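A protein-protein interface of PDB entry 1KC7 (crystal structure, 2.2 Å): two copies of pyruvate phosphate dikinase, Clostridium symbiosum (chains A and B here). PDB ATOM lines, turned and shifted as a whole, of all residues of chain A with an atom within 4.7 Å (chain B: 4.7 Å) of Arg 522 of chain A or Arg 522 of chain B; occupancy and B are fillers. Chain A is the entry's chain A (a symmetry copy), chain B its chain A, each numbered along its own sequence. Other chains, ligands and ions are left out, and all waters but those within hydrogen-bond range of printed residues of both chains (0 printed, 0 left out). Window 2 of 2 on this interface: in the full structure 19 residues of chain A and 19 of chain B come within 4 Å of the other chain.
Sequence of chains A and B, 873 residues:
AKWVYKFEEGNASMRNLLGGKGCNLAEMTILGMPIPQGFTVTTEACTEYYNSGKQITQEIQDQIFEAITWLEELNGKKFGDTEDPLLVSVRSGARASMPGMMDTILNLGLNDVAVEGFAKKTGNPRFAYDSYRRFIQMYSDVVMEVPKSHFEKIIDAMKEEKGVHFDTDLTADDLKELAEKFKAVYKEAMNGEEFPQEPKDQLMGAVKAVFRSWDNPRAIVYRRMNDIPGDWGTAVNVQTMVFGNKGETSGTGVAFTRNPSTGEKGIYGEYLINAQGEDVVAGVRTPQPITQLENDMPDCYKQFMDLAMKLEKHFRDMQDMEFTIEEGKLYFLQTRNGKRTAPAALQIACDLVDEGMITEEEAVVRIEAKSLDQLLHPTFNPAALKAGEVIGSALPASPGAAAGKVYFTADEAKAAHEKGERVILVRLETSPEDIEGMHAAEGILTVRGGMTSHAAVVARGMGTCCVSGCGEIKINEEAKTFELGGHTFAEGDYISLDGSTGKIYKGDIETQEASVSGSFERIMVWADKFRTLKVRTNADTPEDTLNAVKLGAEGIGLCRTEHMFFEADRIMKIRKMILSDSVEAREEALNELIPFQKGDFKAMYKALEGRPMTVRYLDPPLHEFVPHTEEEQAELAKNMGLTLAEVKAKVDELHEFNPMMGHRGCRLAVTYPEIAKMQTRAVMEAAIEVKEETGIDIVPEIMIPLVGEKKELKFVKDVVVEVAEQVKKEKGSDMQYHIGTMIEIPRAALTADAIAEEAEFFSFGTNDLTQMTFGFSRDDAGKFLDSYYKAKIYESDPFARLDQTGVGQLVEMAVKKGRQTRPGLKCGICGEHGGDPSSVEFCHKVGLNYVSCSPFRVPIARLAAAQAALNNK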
ATOM      1  N   CYS A 350      25.563   0.875  -4.415  1.00  0.00           N
ATOM      2  CA  CYS A 350      24.712   0.638  -3.277  1.00  0.00           C
ATOM      3  C   CYS A 350      23.966   1.884  -2.776  1.00  0.00           C
ATOM      4  O   CYS A 350      22.805   1.774  -2.367  1.00  0.00           O
ATOM      5  CB  CYS A 350      25.515  -0.018  -2.172  1.00  0.00           C
ATOM      6  SG  CYS A 350      25.645  -1.795  -2.469  1.00  0.00           S
ATOM      7  N   ASP A 354      19.898   2.554  -2.679  1.00  0.00           N
ATOM      8  CA  ASP A 354      19.207   3.006  -1.484  1.00  0.00           C
ATOM      9  C   ASP A 354      18.441   4.355  -1.633  1.00  0.00           C
ATOM     10  O   ASP A 354      17.562   4.638  -0.838  1.00  0.00           O
ATOM     11  CB  ASP A 354      20.213   3.133  -0.333  1.00  0.00           C
ATOM     12  CG  ASP A 354      20.827   1.777   0.093  1.00  0.00           C
ATOM     13  OD1 ASP A 354      20.189   0.756  -0.192  1.00  0.00           O
ATOM     14  OD2 ASP A 354      21.931   1.735   0.737  1.00  0.00           O
ATOM     15  N   SER A 519      28.482  -3.967   1.086  1.00  0.00           N
ATOM     16  CA  SER A 519      28.197  -3.413  -0.233  1.00  0.00           C
ATOM     17  C   SER A 519      28.933  -4.370  -1.175  1.00  0.00           C
ATOM     18  O   SER A 519      28.534  -4.506  -2.336  1.00  0.00           O
ATOM     19  CB  SER A 519      28.669  -1.950  -0.391  1.00  0.00           C
ATOM     20  OG  SER A 519      27.560  -1.065  -0.557  1.00  0.00           O
ATOM     21  N   PHE A 520      30.013  -5.009  -0.686  1.00  0.00           N
ATOM     22  CA  PHE A 520      30.651  -6.069  -1.495  1.00  0.00           C
ATOM     23  C   PHE A 520      29.691  -7.251  -1.234  1.00  0.00           C
ATOM     24  O   PHE A 520      29.110  -7.840  -2.154  1.00  0.00           O
ATOM     25  CB  PHE A 520      32.050  -6.507  -1.010  1.00  0.00           C
ATOM     26  CG  PHE A 520      32.441  -7.890  -1.516  1.00  0.00           C
ATOM     27  CD1 PHE A 520      32.823  -8.085  -2.842  1.00  0.00           C
ATOM     28  CD2 PHE A 520      32.272  -9.008  -0.721  1.00  0.00           C
ATOM     29  CE1 PHE A 520      33.011  -9.360  -3.364  1.00  0.00           C
ATOM     30  CE2 PHE A 520      32.462 -10.285  -1.240  1.00  0.00           C
ATOM     31  CZ  PHE A 520      32.828 -10.462  -2.568  1.00  0.00           C
ATOM     32  N   GLU A 521      29.514  -7.556   0.048  1.00  0.00           N
ATOM     33  CA  GLU A 521      28.638  -8.637   0.492  1.00  0.00           C
ATOM     34  C   GLU A 521      27.241  -8.379  -0.008  1.00  0.00           C
ATOM     35  O   GLU A 521      26.478  -9.305  -0.239  1.00  0.00           O
ATOM     36  CB  GLU A 521      28.625  -8.677   2.006  1.00  0.00           C
ATOM     37  CG  GLU A 521      30.009  -8.799   2.606  1.00  0.00           C
ATOM     38  CD  GLU A 521      30.545 -10.193   2.528  1.00  0.00           C
ATOM     39  OE1 GLU A 521      30.467 -10.784   1.432  1.00  0.00           O
ATOM     40  OE2 GLU A 521      31.037 -10.699   3.556  1.00  0.00           O
ATOM     41  N   ARG A 522      26.931  -7.113  -0.238  1.00  0.00           N
ATOM     42  CA  ARG A 522      25.593  -6.747  -0.673  1.00  0.00           C
ATOM     43  C   ARG A 522      25.376  -6.950  -2.133  1.00  0.00           C
ATOM     44  O   ARG A 522      24.272  -7.374  -2.565  1.00  0.00           O
ATOM     45  CB  ARG A 522      25.286  -5.278  -0.325  1.00  0.00           C
ATOM     46  CG  ARG A 522      24.917  -5.022   1.133  1.00  0.00           C
ATOM     47  CD  ARG A 522      24.398  -3.571   1.326  1.00  0.00           C
ATOM     48  NE  ARG A 522      23.028  -3.349   0.822  1.00  0.00           N
ATOM     49  CZ  ARG A 522      22.505  -2.136   0.624  1.00  0.00           C
ATOM     50  NH1 ARG A 522      23.234  -1.067   0.875  1.00  0.00           N
ATOM     51  NH2 ARG A 522      21.241  -1.977   0.212  1.00  0.00           N
ATOM     52  N   ILE A 523      26.405  -6.623  -2.911  1.00  0.00           N
ATOM     53  CA  ILE A 523      26.319  -6.780  -4.361  1.00  0.00           C
ATOM     54  C   ILE A 523      26.334  -8.295  -4.602  1.00  0.00           C
ATOM     55  O   ILE A 523      25.557  -8.831  -5.421  1.00  0.00           O
ATOM     56  CB  ILE A 523      27.495  -6.019  -5.063  1.00  0.00           C
ATOM     57  CG1 ILE A 523      27.292  -4.509  -4.874  1.00  0.00           C
ATOM     58  CG2 ILE A 523      27.541  -6.321  -6.555  1.00  0.00           C
ATOM     59  CD1 ILE A 523      26.071  -3.958  -5.557  1.00  0.00           C
ATOM     60  N   MET A 524      27.209  -8.979  -3.863  1.00  0.00           N
ATOM     61  CA  MET A 524      27.271 -10.439  -3.928  1.00  0.00           C
ATOM     62  C   MET A 524      25.885 -11.063  -3.658  1.00  0.00           C
ATOM     63  O   MET A 524      25.475 -11.966  -4.363  1.00  0.00           O
ATOM     64  CB  MET A 524      28.291 -10.958  -2.910  1.00  0.00           C
ATOM     65  CG  MET A 524      29.719 -10.549  -3.295  1.00  0.00           C
ATOM     66  SD  MET A 524      30.187 -11.413  -4.889  1.00  0.00           S
ATOM     67  CE  MET A 524      30.257 -10.022  -6.039  1.00  0.00           C
ATOM     68  N   VAL A 525      25.133 -10.559  -2.685  1.00  0.00           N
ATOM     69  CA  VAL A 525      23.824 -11.148  -2.396  1.00  0.00           C
ATOM     70  C   VAL A 525      22.887 -10.847  -3.533  1.00  0.00           C
ATOM     71  O   VAL A 525      21.966 -11.612  -3.803  1.00  0.00           O
ATOM     72  CB  VAL A 525      23.214 -10.612  -1.050  1.00  0.00           C
ATOM     73  CG1 VAL A 525      21.698 -10.750  -1.064  1.00  0.00           C
ATOM     74  CG2 VAL A 525      23.774 -11.408   0.124  1.00  0.00           C
ATOM     75  N   TRP A 526      23.120  -9.722  -4.197  1.00  0.00           N
ATOM     76  CA  TRP A 526      22.308  -9.361  -5.345  1.00  0.00           C
ATOM     77  C   TRP A 526      22.808 -10.185  -6.536  1.00  0.00           C
ATOM     78  O   TRP A 526      22.012 -10.678  -7.325  1.00  0.00           O
ATOM     79  CB  TRP A 526      22.400  -7.855  -5.635  1.00  0.00           C
ATOM     80  CG  TRP A 526      21.814  -6.965  -4.535  1.00  0.00           C
ATOM     81  CD1 TRP A 526      21.152  -7.364  -3.397  1.00  0.00           C
ATOM     82  CD2 TRP A 526      21.903  -5.540  -4.458  1.00  0.00           C
ATOM     83  NE1 TRP A 526      20.834  -6.273  -2.618  1.00  0.00           N
ATOM     84  CE2 TRP A 526      21.285  -5.143  -3.240  1.00  0.00           C
ATOM     85  CE3 TRP A 526      22.452  -4.553  -5.296  1.00  0.00           C
ATOM     86  CZ2 TRP A 526      21.204  -3.821  -2.845  1.00  0.00           C
ATOM     87  CZ3 TRP A 526      22.366  -3.228  -4.900  1.00  0.00           C
ATOM     88  CH2 TRP A 526      21.750  -2.874  -3.688  1.00  0.00           C
ATOM     89  N   CYS B 350      20.076 -11.811   8.314  1.00  0.00           N
ATOM     90  CA  CYS B 350      20.139 -11.503   6.909  1.00  0.00           C
ATOM     91  C   CYS B 350      19.655 -12.635   5.991  1.00  0.00           C
ATOM     92  O   CYS B 350      19.015 -12.359   4.970  1.00  0.00           O
ATOM     93  CB  CYS B 350      21.540 -11.050   6.552  1.00  0.00           C
ATOM     94  SG  CYS B 350      21.753  -9.304   6.965  1.00  0.00           S
ATOM     95  N   ASP B 354      16.431 -12.634   3.419  1.00  0.00           N
ATOM     96  CA  ASP B 354      16.540 -13.033   2.027  1.00  0.00           C
ATOM     97  C   ASP B 354      15.631 -14.227   1.607  1.00  0.00           C
ATOM     98  O   ASP B 354      15.380 -14.407   0.429  1.00  0.00           O
ATOM     99  CB  ASP B 354      17.999 -13.387   1.712  1.00  0.00           C
ATOM    100  CG  ASP B 354      18.958 -12.175   1.820  1.00  0.00           C
ATOM    101  OD1 ASP B 354      18.455 -11.050   1.718  1.00  0.00           O
ATOM    102  OD2 ASP B 354      20.215 -12.350   1.977  1.00  0.00           O
ATOM    103  N   SER B 519      26.469  -7.826   5.973  1.00  0.00           N
ATOM    104  CA  SER B 519      25.358  -8.253   6.819  1.00  0.00           C
ATOM    105  C   SER B 519      25.520  -7.377   8.065  1.00  0.00           C
ATOM    106  O   SER B 519      24.530  -7.114   8.755  1.00  0.00           O
ATOM    107  CB  SER B 519      25.392  -9.762   7.148  1.00  0.00           C
ATOM    108  OG  SER B 519      24.282 -10.442   6.562  1.00  0.00           O
ATOM    109  N   PHE B 520      26.763  -6.953   8.364  1.00  0.00           N
ATOM    110  CA  PHE B 520      26.945  -5.968   9.453  1.00  0.00           C
ATOM    111  C   PHE B 520      26.547  -4.661   8.730  1.00  0.00           C
ATOM    112  O   PHE B 520      25.636  -3.934   9.144  1.00  0.00           O
ATOM    113  CB  PHE B 520      28.401  -5.792   9.936  1.00  0.00           C
ATOM    114  CG  PHE B 520      28.627  -4.467  10.651  1.00  0.00           C
ATOM    115  CD1 PHE B 520      28.156  -4.263  11.947  1.00  0.00           C
ATOM    116  CD2 PHE B 520      29.159  -3.382   9.979  1.00  0.00           C
ATOM    117  CE1 PHE B 520      28.196  -3.009  12.547  1.00  0.00           C
ATOM    118  CE2 PHE B 520      29.202  -2.126  10.578  1.00  0.00           C
ATOM    119  CZ  PHE B 520      28.715  -1.939  11.864  1.00  0.00           C
ATOM    120  N   GLU B 521      27.234  -4.403   7.621  1.00  0.00           N
ATOM    121  CA  GLU B 521      26.996  -3.220   6.799  1.00  0.00           C
ATOM    122  C   GLU B 521      25.563  -3.217   6.338  1.00  0.00           C
ATOM    123  O   GLU B 521      24.979  -2.168   6.113  1.00  0.00           O
ATOM    124  CB  GLU B 521      27.907  -3.263   5.590  1.00  0.00           C
ATOM    125  CG  GLU B 521      29.369  -3.402   5.955  1.00  0.00           C
ATOM    126  CD  GLU B 521      29.968  -2.112   6.419  1.00  0.00           C
ATOM    127  OE1 GLU B 521      29.342  -1.457   7.276  1.00  0.00           O
ATOM    128  OE2 GLU B 521      31.056  -1.752   5.926  1.00  0.00           O
ATOM    129  N   ARG B 522      24.975  -4.400   6.264  1.00  0.00           N
ATOM    130  CA  ARG B 522      23.608  -4.518   5.781  1.00  0.00           C
ATOM    131  C   ARG B 522      22.590  -4.201   6.822  1.00  0.00           C
ATOM    132  O   ARG B 522      21.538  -3.579   6.522  1.00  0.00           O
ATOM    133  CB  ARG B 522      23.338  -5.934   5.238  1.00  0.00           C
ATOM    134  CG  ARG B 522      23.889  -6.207   3.841  1.00  0.00           C
ATOM    135  CD  ARG B 522      23.363  -7.561   3.293  1.00  0.00           C
ATOM    136  NE  ARG B 522      21.954  -7.527   2.855  1.00  0.00           N
ATOM    137  CZ  ARG B 522      21.228  -8.625   2.628  1.00  0.00           C
ATOM    138  NH1 ARG B 522      21.772  -9.811   2.810  1.00  0.00           N
ATOM    139  NH2 ARG B 522      19.967  -8.552   2.183  1.00  0.00           N
ATOM    140  N   ILE B 523      22.869  -4.648   8.043  1.00  0.00           N
ATOM    141  CA  ILE B 523      21.952  -4.399   9.153  1.00  0.00           C
ATOM    142  C   ILE B 523      22.066  -2.896   9.438  1.00  0.00           C
ATOM    143  O   ILE B 523      21.053  -2.195   9.650  1.00  0.00           O
ATOM    144  CB  ILE B 523      22.320  -5.302  10.380  1.00  0.00           C
ATOM    145  CG1 ILE B 523      22.029  -6.766  10.023  1.00  0.00           C
ATOM    146  CG2 ILE B 523      21.505  -4.930  11.611  1.00  0.00           C
ATOM    147  CD1 ILE B 523      20.574  -7.072   9.798  1.00  0.00           C
ATOM    148  N   MET B 524      23.307  -2.407   9.417  1.00  0.00           N
ATOM    149  CA  MET B 524      23.556  -0.975   9.587  1.00  0.00           C
ATOM    150  C   MET B 524      22.740  -0.149   8.571  1.00  0.00           C
ATOM    151  O   MET B 524      22.142   0.847   8.934  1.00  0.00           O
ATOM    152  CB  MET B 524      25.051  -0.687   9.423  1.00  0.00           C
ATOM    153  CG  MET B 524      25.865  -1.303  10.569  1.00  0.00           C
ATOM    154  SD  MET B 524      25.409  -0.440  12.167  1.00  0.00           S
ATOM    155  CE  MET B 524      24.541  -1.758  13.047  1.00  0.00           C
ATOM    156  N   VAL B 525      22.658  -0.576   7.314  1.00  0.00           N
ATOM    157  CA  VAL B 525      21.908   0.203   6.327  1.00  0.00           C
ATOM    158  C   VAL B 525      20.441   0.123   6.648  1.00  0.00           C
ATOM    159  O   VAL B 525      19.685   1.042   6.349  1.00  0.00           O
ATOM    160  CB  VAL B 525      22.158  -0.300   4.859  1.00  0.00           C
ATOM    161  CG1 VAL B 525      20.989   0.085   3.962  1.00  0.00           C
ATOM    162  CG2 VAL B 525      23.434   0.327   4.308  1.00  0.00           C
ATOM    163  N   TRP B 526      20.037  -0.987   7.254  1.00  0.00           N
ATOM    164  CA  TRP B 526      18.651  -1.145   7.656  1.00  0.00           C
ATOM    165  C   TRP B 526      18.457  -0.350   8.951  1.00  0.00           C
ATOM    166  O   TRP B 526      17.441   0.310   9.125  1.00  0.00           O
ATOM    167  CB  TRP B 526      18.302  -2.627   7.859  1.00  0.00           C
ATOM    168  CG  TRP B 526      18.363  -3.470   6.582  1.00  0.00           C
ATOM    169  CD1 TRP B 526      18.600  -3.031   5.299  1.00  0.00           C
ATOM    170  CD2 TRP B 526      18.246  -4.892   6.494  1.00  0.00           C
ATOM    171  NE1 TRP B 526      18.644  -4.098   4.426  1.00  0.00           N
ATOM    172  CE2 TRP B 526      18.435  -5.249   5.130  1.00  0.00           C
ATOM    173  CE3 TRP B 526      18.007  -5.908   7.437  1.00  0.00           C
ATOM    174  CZ2 TRP B 526      18.393  -6.561   4.694  1.00  0.00           C
ATOM    175  CZ3 TRP B 526      17.961  -7.221   6.997  1.00  0.00           C
ATOM    176  CH2 TRP B 526      18.156  -7.536   5.642  1.00  0.00           C
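The side-chain carboxylate (OD1) of Asp 354 of chain B is in salt-bridge range of the guanidinium group (NH2) of Arg 522 of chain B.
The side-chain carboxylate (OD1) of Asp 354 of chain A lies within salt-bridge range of the guanidinium group (NH2) of Arg 522 of chain A, at 3.0 Å.
Asp 354 of chain A touches Val 525 of chain B (OD2 to CG1, 3.7 Å).
CG of Arg 522 of chain B touches CG of Arg 522 of chain A (3.1 Å).
Arg 522 of chain A touches Val 525 of chain B.
CG1 of Val 525 of chain A touches OD2 of Asp 354 of chain B, 3.7 Å away.
CG2 of Val 525 of chain A touches NH1 of Arg 522 of chain B, 3.7 Å away.
Of chain B, only Arg 522 and Val 525 come within 4 Å of Arg 522 of chain A.
Arg 522 of chain B touches just these residues of chain A: Arg 522 (3.1 Å) and Val 525 (3.7 Å).
Of the printed residues of chain A, Val 525 of chain B touches Asp 354 (3.7 Å) and Arg 522 (3.7 Å).
Of the printed residues of chain B, Val 525 of chain A touches Asp 354 (3.7 Å) and Arg 522 (3.7 Å).
Of the printed residues of chain A, Asp 354 of chain B touches Val 525.
Of the printed residues of chain B, Asp 354 of chain A touches Val 525.
Of the 10 printed residues of chain A, 3 touch a printed residue of chain B.
Hydrophobic or aromatic side chains of chain A within 4 Å of the printed part of chain B: Val 525.
Of the 10 printed residues of chain B, 3 touch a printed residue of chain A.
Among the printed residues, 5 pairs touch across the chains.
Among the printed residues, no Asp or Glu carboxylate lies within 4 Å of a Lys or Arg side-chain nitrogen of the other chain.
Asp 354 of chain A touches Val 525 of chain B, and with the chains exchanged Val 525 of chain A touches Asp 354 of chain B.
Arg 522 of chain A touches its own counterpart, Arg 522 of chain B.
Arg 522 of chain A touches Val 525 of chain B, and with the chains exchanged Val 525 of chain A touches Arg 522 of chain B.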
